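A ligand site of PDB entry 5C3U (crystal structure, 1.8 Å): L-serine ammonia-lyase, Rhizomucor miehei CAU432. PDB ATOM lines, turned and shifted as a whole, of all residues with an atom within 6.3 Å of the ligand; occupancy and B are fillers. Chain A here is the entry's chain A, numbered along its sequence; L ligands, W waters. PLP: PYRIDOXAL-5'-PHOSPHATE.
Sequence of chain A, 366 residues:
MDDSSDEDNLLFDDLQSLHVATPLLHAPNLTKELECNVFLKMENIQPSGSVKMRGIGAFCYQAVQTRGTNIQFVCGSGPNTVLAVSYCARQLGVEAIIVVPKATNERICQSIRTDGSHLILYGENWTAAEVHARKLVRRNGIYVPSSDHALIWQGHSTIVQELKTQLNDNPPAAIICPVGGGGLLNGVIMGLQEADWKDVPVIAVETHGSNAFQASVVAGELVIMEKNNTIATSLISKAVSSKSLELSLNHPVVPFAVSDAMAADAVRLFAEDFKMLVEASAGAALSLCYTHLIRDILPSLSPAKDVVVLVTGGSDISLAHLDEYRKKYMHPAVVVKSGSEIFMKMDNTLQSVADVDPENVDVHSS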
ATOM      1  N   SER A  50      22.043  12.679   7.097  1.00  0.00           N
ATOM      2  CA  SER A  50      20.719  13.288   7.347  1.00  0.00           C
ATOM      3  C   SER A  50      20.727  14.406   8.364  1.00  0.00           C
ATOM      4  O   SER A  50      21.730  14.622   9.063  1.00  0.00           O
ATOM      5  CB  SER A  50      19.726  12.206   7.781  1.00  0.00           C
ATOM      6  OG  SER A  50      19.799  12.011   9.185  1.00  0.00           O
ATOM      7  N   VAL A  51      19.596  15.108   8.453  1.00  0.00           N
ATOM      8  CA  VAL A  51      19.349  16.172   9.434  1.00  0.00           C
ATOM      9  C   VAL A  51      19.540  15.713  10.905  1.00  0.00           C
ATOM     10  O   VAL A  51      19.814  16.541  11.765  1.00  0.00           O
ATOM     11  CB  VAL A  51      17.928  16.792   9.243  1.00  0.00           C
ATOM     12  CG1 VAL A  51      16.821  15.825   9.680  1.00  0.00           C
ATOM     13  CG2 VAL A  51      17.802  18.140   9.944  1.00  0.00           C
ATOM     14  N   LYS A  52      19.418  14.400  11.165  1.00  0.00           N
ATOM     15  CA  LYS A  52      19.606  13.862  12.512  1.00  0.00           C
ATOM     16  C   LYS A  52      20.911  14.284  13.127  1.00  0.00           C
ATOM     17  O   LYS A  52      21.018  14.439  14.351  1.00  0.00           O
ATOM     18  CB  LYS A  52      19.468  12.330  12.592  1.00  0.00           C
ATOM     19  CG  LYS A  52      18.059  11.813  12.272  1.00  0.00           C
ATOM     20  CD  LYS A  52      17.110  12.304  13.372  1.00  0.00           C
ATOM     21  CE  LYS A  52      15.825  11.511  13.388  1.00  0.00           C
ATOM     22  NZ  LYS A  52      15.237  11.479  12.025  1.00  0.00           N
ATOM     23  N   ASN A  80      18.029   6.754  10.487  1.00  0.00           N
ATOM     24  CA  ASN A  80      18.946   7.895  10.496  1.00  0.00           C
ATOM     25  C   ASN A  80      19.412   8.241  11.885  1.00  0.00           C
ATOM     26  O   ASN A  80      20.509   8.784  12.046  1.00  0.00           O
ATOM     27  CB  ASN A  80      18.348   9.051   9.753  1.00  0.00           C
ATOM     28  CG  ASN A  80      18.017   8.656   8.319  1.00  0.00           C
ATOM     29  OD1 ASN A  80      18.910   8.138   7.615  1.00  0.00           O
ATOM     30  ND2 ASN A  80      16.773   8.828   7.911  1.00  0.00           N
ATOM     31  N   THR A  81      18.585   7.929  12.886  1.00  0.00           N
ATOM     32  CA  THR A  81      18.995   8.129  14.268  1.00  0.00           C
ATOM     33  C   THR A  81      20.167   7.207  14.607  1.00  0.00           C
ATOM     34  O   THR A  81      21.182   7.676  15.136  1.00  0.00           O
ATOM     35  CB  THR A  81      17.837   7.919  15.236  1.00  0.00           C
ATOM     36  OG1 THR A  81      16.719   8.652  14.730  1.00  0.00           O
ATOM     37  CG2 THR A  81      18.206   8.435  16.650  1.00  0.00           C
ATOM     38  N   SER A 146      14.788   9.508  19.040  1.00  0.00           N
ATOM     39  CA  SER A 146      14.921  10.110  17.717  1.00  0.00           C
ATOM     40  C   SER A 146      14.456  11.580  17.700  1.00  0.00           C
ATOM     41  O   SER A 146      14.932  12.361  16.874  1.00  0.00           O
ATOM     42  CB  SER A 146      14.125   9.286  16.692  1.00  0.00           C
ATOM     43  OG  SER A 146      12.739   9.365  16.994  1.00  0.00           O
ATOM     44  N   SER A 147      13.518  11.944  18.570  1.00  0.00           N
ATOM     45  CA  SER A 147      12.764  13.191  18.397  1.00  0.00           C
ATOM     46  C   SER A 147      12.434  13.959  19.682  1.00  0.00           C
ATOM     47  O   SER A 147      12.572  15.179  19.708  1.00  0.00           O
ATOM     48  CB  SER A 147      11.432  12.896  17.663  1.00  0.00           C
ATOM     49  OG  SER A 147      11.620  12.039  16.548  1.00  0.00           O
ATOM     50  N   ILE A 152      17.602  17.645  21.451  1.00  0.00           N
ATOM     51  CA  ILE A 152      17.367  17.391  20.017  1.00  0.00           C
ATOM     52  C   ILE A 152      16.734  18.631  19.382  1.00  0.00           C
ATOM     53  O   ILE A 152      17.160  19.089  18.322  1.00  0.00           O
ATOM     54  CB  ILE A 152      16.512  16.131  19.827  1.00  0.00           C
ATOM     55  CG1 ILE A 152      17.252  14.893  20.382  1.00  0.00           C
ATOM     56  CG2 ILE A 152      16.169  15.925  18.351  1.00  0.00           C
ATOM     57  CD1 ILE A 152      16.480  13.601  20.271  1.00  0.00           C
ATOM     58  N   HIS A 156      18.441  20.823  16.403  1.00  0.00           N
ATOM     59  CA  HIS A 156      17.758  21.079  15.145  1.00  0.00           C
ATOM     60  C   HIS A 156      17.566  22.544  14.883  1.00  0.00           C
ATOM     61  O   HIS A 156      17.544  22.961  13.729  1.00  0.00           O
ATOM     62  CB  HIS A 156      16.428  20.366  15.073  1.00  0.00           C
ATOM     63  CG  HIS A 156      16.521  18.855  14.821  1.00  0.00           C
ATOM     64  ND1 HIS A 156      17.473  18.291  14.009  1.00  0.00           N
ATOM     65  CD2 HIS A 156      15.728  17.815  15.277  1.00  0.00           C
ATOM     66  CE1 HIS A 156      17.283  16.957  13.985  1.00  0.00           C
ATOM     67  NE2 HIS A 156      16.193  16.676  14.731  1.00  0.00           N
ATOM     68  N   PRO A 178       9.266  18.042   6.908  1.00  0.00           N
ATOM     69  CA  PRO A 178       8.715  16.697   7.151  1.00  0.00           C
ATOM     70  C   PRO A 178       8.541  16.460   8.659  1.00  0.00           C
ATOM     71  O   PRO A 178       9.381  16.930   9.434  1.00  0.00           O
ATOM     72  CB  PRO A 178       9.783  15.731   6.592  1.00  0.00           C
ATOM     73  CG  PRO A 178      10.943  16.578   6.239  1.00  0.00           C
ATOM     74  CD  PRO A 178      10.655  18.029   6.409  1.00  0.00           C
ATOM     75  N   VAL A 179       7.457  15.773   9.063  1.00  0.00           N
ATOM     76  CA  VAL A 179       7.211  15.449  10.483  1.00  0.00           C
ATOM     77  C   VAL A 179       7.082  13.938  10.734  1.00  0.00           C
ATOM     78  O   VAL A 179       6.243  13.268  10.115  1.00  0.00           O
ATOM     79  CB  VAL A 179       5.952  16.194  11.046  1.00  0.00           C
ATOM     80  CG1 VAL A 179       5.702  15.822  12.507  1.00  0.00           C
ATOM     81  CG2 VAL A 179       6.152  17.696  10.916  1.00  0.00           C
ATOM     82  N   GLY A 180       7.963  13.416  11.605  1.00  0.00           N
ATOM     83  CA  GLY A 180       7.871  12.057  12.169  1.00  0.00           C
ATOM     84  C   GLY A 180       7.359  12.169  13.590  1.00  0.00           C
ATOM     85  O   GLY A 180       6.145  12.216  13.807  1.00  0.00           O
ATOM     86  N   GLY A 181       8.276  12.270  14.558  1.00  0.00           N
ATOM     87  CA  GLY A 181       7.874  12.489  15.956  1.00  0.00           C
ATOM     88  C   GLY A 181       7.816  13.946  16.374  1.00  0.00           C
ATOM     89  O   GLY A 181       7.412  14.252  17.504  1.00  0.00           O
ATOM     90  N   GLY A 182       8.232  14.844  15.474  1.00  0.00           N
ATOM     91  CA  GLY A 182       8.160  16.277  15.709  1.00  0.00           C
ATOM     92  C   GLY A 182       9.405  16.980  16.239  1.00  0.00           C
ATOM     93  O   GLY A 182       9.344  18.175  16.531  1.00  0.00           O
ATOM     94  N   GLY A 183      10.530  16.265  16.346  1.00  0.00           N
ATOM     95  CA  GLY A 183      11.786  16.866  16.820  1.00  0.00           C
ATOM     96  C   GLY A 183      12.280  17.997  15.935  1.00  0.00           C
ATOM     97  O   GLY A 183      12.650  19.068  16.418  1.00  0.00           O
ATOM     98  N   LEU A 184      12.321  17.742  14.631  1.00  0.00           N
ATOM     99  CA  LEU A 184      12.795  18.742  13.662  1.00  0.00           C
ATOM    100  C   LEU A 184      11.834  19.922  13.642  1.00  0.00           C
ATOM    101  O   LEU A 184      12.245  21.077  13.756  1.00  0.00           O
ATOM    102  CB  LEU A 184      12.936  18.127  12.278  1.00  0.00           C
ATOM    103  CG  LEU A 184      13.374  19.049  11.151  1.00  0.00           C
ATOM    104  CD1 LEU A 184      14.718  19.726  11.439  1.00  0.00           C
ATOM    105  CD2 LEU A 184      13.409  18.245   9.857  1.00  0.00           C
ATOM    106  N   LEU A 185      10.558  19.596  13.546  1.00  0.00           N
ATOM    107  CA  LEU A 185       9.501  20.591  13.642  1.00  0.00           C
ATOM    108  C   LEU A 185       9.704  21.530  14.835  1.00  0.00           C
ATOM    109  O   LEU A 185       9.678  22.755  14.663  1.00  0.00           O
ATOM    110  CB  LEU A 185       8.133  19.919  13.709  1.00  0.00           C
ATOM    111  CG  LEU A 185       7.005  20.947  13.858  1.00  0.00           C
ATOM    112  CD1 LEU A 185       6.971  21.874  12.646  1.00  0.00           C
ATOM    113  CD2 LEU A 185       5.655  20.288  14.100  1.00  0.00           C
ATOM    114  N   SER A 234      11.198   7.251   8.179  1.00  0.00           N
ATOM    115  CA  SER A 234      11.592   8.127   9.277  1.00  0.00           C
ATOM    116  C   SER A 234      10.423   8.961   9.782  1.00  0.00           C
ATOM    117  O   SER A 234      10.546   9.618  10.808  1.00  0.00           O
ATOM    118  CB  SER A 234      12.771   9.006   8.919  1.00  0.00           C
ATOM    119  OG  SER A 234      13.884   8.168   8.621  1.00  0.00           O
ATOM    120  N   LEU A 235       9.309   8.903   9.077  1.00  0.00           N
ATOM    121  CA  LEU A 235       8.104   9.654   9.495  1.00  0.00           C
ATOM    122  C   LEU A 235       7.123   8.808  10.278  1.00  0.00           C
ATOM    123  O   LEU A 235       6.110   9.334  10.781  1.00  0.00           O
ATOM    124  CB  LEU A 235       7.416  10.312   8.287  1.00  0.00           C
ATOM    125  CG  LEU A 235       8.252  11.271   7.412  1.00  0.00           C
ATOM    126  CD1 LEU A 235       7.407  12.068   6.419  1.00  0.00           C
ATOM    127  CD2 LEU A 235       9.173  12.206   8.223  1.00  0.00           C
ATOM    128  N   GLU A 279      15.522   9.964   0.983  1.00  0.00           N
ATOM    129  CA  GLU A 279      14.468   9.078   1.493  1.00  0.00           C
ATOM    130  C   GLU A 279      13.104   9.638   1.136  1.00  0.00           C
ATOM    131  O   GLU A 279      12.966  10.844   0.950  1.00  0.00           O
ATOM    132  CB  GLU A 279      14.535   9.042   3.003  1.00  0.00           C
ATOM    133  CG  GLU A 279      15.280   7.879   3.558  1.00  0.00           C
ATOM    134  CD  GLU A 279      15.275   7.850   5.080  1.00  0.00           C
ATOM    135  OE1 GLU A 279      14.221   8.131   5.725  1.00  0.00           O
ATOM    136  OE2 GLU A 279      16.332   7.537   5.616  1.00  0.00           O
ATOM    137  N   SER A 281      10.845  10.117   3.169  1.00  0.00           N
ATOM    138  CA  SER A 281      10.607  11.142   4.183  1.00  0.00           C
ATOM    139  C   SER A 281      10.850  12.575   3.655  1.00  0.00           C
ATOM    140  O   SER A 281       9.998  13.462   3.780  1.00  0.00           O
ATOM    141  CB  SER A 281      11.475  10.854   5.428  1.00  0.00           C
ATOM    142  OG  SER A 281      11.296   9.485   5.812  1.00  0.00           O
ATOM    143  N   ALA A 282      12.009  12.786   3.024  1.00  0.00           N
ATOM    144  CA  ALA A 282      12.327  14.084   2.435  1.00  0.00           C
ATOM    145  C   ALA A 282      11.482  14.282   1.189  1.00  0.00           C
ATOM    146  O   ALA A 282      11.085  15.397   0.858  1.00  0.00           O
ATOM    147  CB  ALA A 282      13.806  14.117   2.055  1.00  0.00           C
ATOM    148  N   THR A 312      15.748  16.594   4.020  1.00  0.00           N
ATOM    149  CA  THR A 312      16.299  15.982   5.236  1.00  0.00           C
ATOM    150  C   THR A 312      17.309  14.870   4.994  1.00  0.00           C
ATOM    151  O   THR A 312      18.058  14.524   5.911  1.00  0.00           O
ATOM    152  CB  THR A 312      15.185  15.556   6.201  1.00  0.00           C
ATOM    153  OG1 THR A 312      14.207  14.776   5.486  1.00  0.00           O
ATOM    154  CG2 THR A 312      14.532  16.799   6.772  1.00  0.00           C
ATOM    155  N   GLY A 313      17.330  14.331   3.769  1.00  0.00           N
ATOM    156  CA  GLY A 313      18.357  13.388   3.361  1.00  0.00           C
ATOM    157  C   GLY A 313      17.900  11.992   3.706  1.00  0.00           C
ATOM    158  O   GLY A 313      16.808  11.556   3.278  1.00  0.00           O
ATOM    159  N   GLY A 314      18.713  11.285   4.473  1.00  0.00           N
ATOM    160  CA  GLY A 314      18.372   9.944   4.940  1.00  0.00           C
ATOM    161  C   GLY A 314      19.062   8.816   4.188  1.00  0.00           C
ATOM    162  O   GLY A 314      19.337   8.922   2.993  1.00  0.00           O
ATOM    163  N   SER A 315      19.295   7.715   4.881  1.00  0.00           N
ATOM    164  CA  SER A 315      20.030   6.590   4.295  1.00  0.00           C
ATOM    165  C   SER A 315      19.154   5.402   3.963  1.00  0.00           C
ATOM    166  O   SER A 315      19.683   4.425   3.434  1.00  0.00           O
ATOM    167  CB  SER A 315      21.192   6.137   5.198  1.00  0.00           C
ATOM    168  OG  SER A 315      22.152   7.190   5.397  1.00  0.00           O
HETATM  169  N1  PLP L   1      13.309  13.152   7.466  1.00  0.00           N
HETATM  170  C2  PLP L   1      14.355  12.357   7.756  1.00  0.00           C
HETATM  171  C2A PLP L   1      15.201  11.724   6.668  1.00  0.00           C
HETATM  172  C3  PLP L   1      14.675  12.078   9.154  1.00  0.00           C
HETATM  173  O3  PLP L   1      15.737  11.272   9.471  1.00  0.00           O
HETATM  174  C4  PLP L   1      13.839  12.731  10.182  1.00  0.00           C
HETATM  175  C4A PLP L   1      14.134  12.517  11.601  1.00  0.00           C
HETATM  176  C5  PLP L   1      12.705  13.595   9.753  1.00  0.00           C
HETATM  177  C6  PLP L   1      12.517  13.760   8.376  1.00  0.00           C
HETATM  178  C5A PLP L   1      11.787  14.298  10.750  1.00  0.00           C
HETATM  179  O4P PLP L   1      11.847  13.599  11.990  1.00  0.00           O
HETATM  180  P   PLP L   1      11.207  14.028  13.416  1.00  0.00           P
HETATM  181  O1P PLP L   1      12.179  14.897  14.118  1.00  0.00           O
HETATM  182  O2P PLP L   1       9.834  14.680  13.171  1.00  0.00           O
HETATM  183  O3P PLP L   1      11.058  12.670  14.010  1.00  0.00           O
HETATM  184  O   HOH W   1      11.889  10.312  12.947  1.00  0.00           O
HETATM  185  O   HOH W   2      14.487  14.462  15.228  1.00  0.00           O
HETATM  186  O   HOH W   3       9.596  17.170  12.424  1.00  0.00           O
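The backbone NH (N) of Gly 181 sits at hydrogen-bond distance from an oxygen (O3P) of the ligand (2.9 Å).
The backbone NH (N) of Gly 183 sits at hydrogen-bond distance from an oxygen (O1P) of the ligand.
The side-chain hydroxyl of Thr 312 lies within hydrogen-bond range of a nitrogen (N1) of the ligand (2.7 Å).
N of Gly 180 is in hydrogen-bond range of O2P of the ligand (2.7 Å).
A carbon (C4A) of the ligand is bonded to the side-chain amino group of Lys 52.
The side-chain amide nitrogen (ND2) of Asn 80 sits at hydrogen-bond distance from an oxygen (O3) of the ligand.
The backbone NH of Leu 184 is in hydrogen-bond range of an oxygen (O1P) of the ligand (2.9 Å).
The backbone NH (N) of Gly 182 sits at hydrogen-bond distance from an oxygen (O2P) of the ligand, 2.8 Å away.
An oxygen (O3P) of the ligand is in hydrogen-bond range of the side-chain hydroxyl of Ser 147, 2.7 Å away.
The side-chain amide nitrogen (ND2) of Asn 80 is in hydrogen-bond range of the side-chain carboxylate (OE2) of Glu 279 (2.7 Å).
N of Glu 279 lies within hydrogen-bond range of O of Gly 313 (3.1 Å).
The side-chain amide nitrogen (ND2) of Asn 80 lies within hydrogen-bond range of the side-chain hydroxyl (OG) of Ser 234.
OD1 of Asn 80 is in hydrogen-bond range of N of Ser 315, at 2.8 Å.
N of Lys 52 lies close to OG of Ser 50 (3.1 Å).
The side-chain hydroxyl (OG) of Ser 146 lies within hydrogen-bond range of the side-chain hydroxyl (OG) of Ser 147 (2.9 Å).
The backbone NH of Ser 234 sits at hydrogen-bond distance from the side-chain hydroxyl of Ser 281, 3.3 Å away.
The backbone carbonyl oxygen (O) of Thr 312 lies within hydrogen-bond range of the backbone NH (N) of Val 51, 3.0 Å away.
Pro 178 touches the ligand (O to C5A, 3.8 Å).
Val 179 touches the ligand (C to O2P, 3.8 Å).
Ser 234 touches the ligand (CB to C3, 3.6 Å).
Leu 235 touches the ligand.
OE1 of Glu 279 touches C2A of the ligand (3.8 Å).
Ser 281 touches the ligand.
O of Gly 313 touches C2A of the ligand (3.8 Å).
Hydrophobic or aromatic side chains within 4 Å of the ligand: Pro 178, Leu 184 and Leu 235.
The nearest printed residue that does not touch the ligand is Gly 314 (4.03 Å).
Water W2 lies within hydrogen-bond range of an oxygen (O1P) of the ligand (2.6 Å), the backbone carbonyl oxygen (O) of Ser 146 (2.7 Å) and a ring nitrogen (NE2) of His 156 (2.8 Å).
Water W3 lies within hydrogen-bond range of an oxygen (O2P) of the ligand (2.6 Å), the backbone NH of Leu 185 (2.8 Å) and the backbone carbonyl oxygen of Pro 178 (3.0 Å).
Water W1 bridges the backbone carbonyl oxygen (O) of Ser 234 (2.6 Å) and an oxygen (O3P) of the ligand (2.7 Å).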
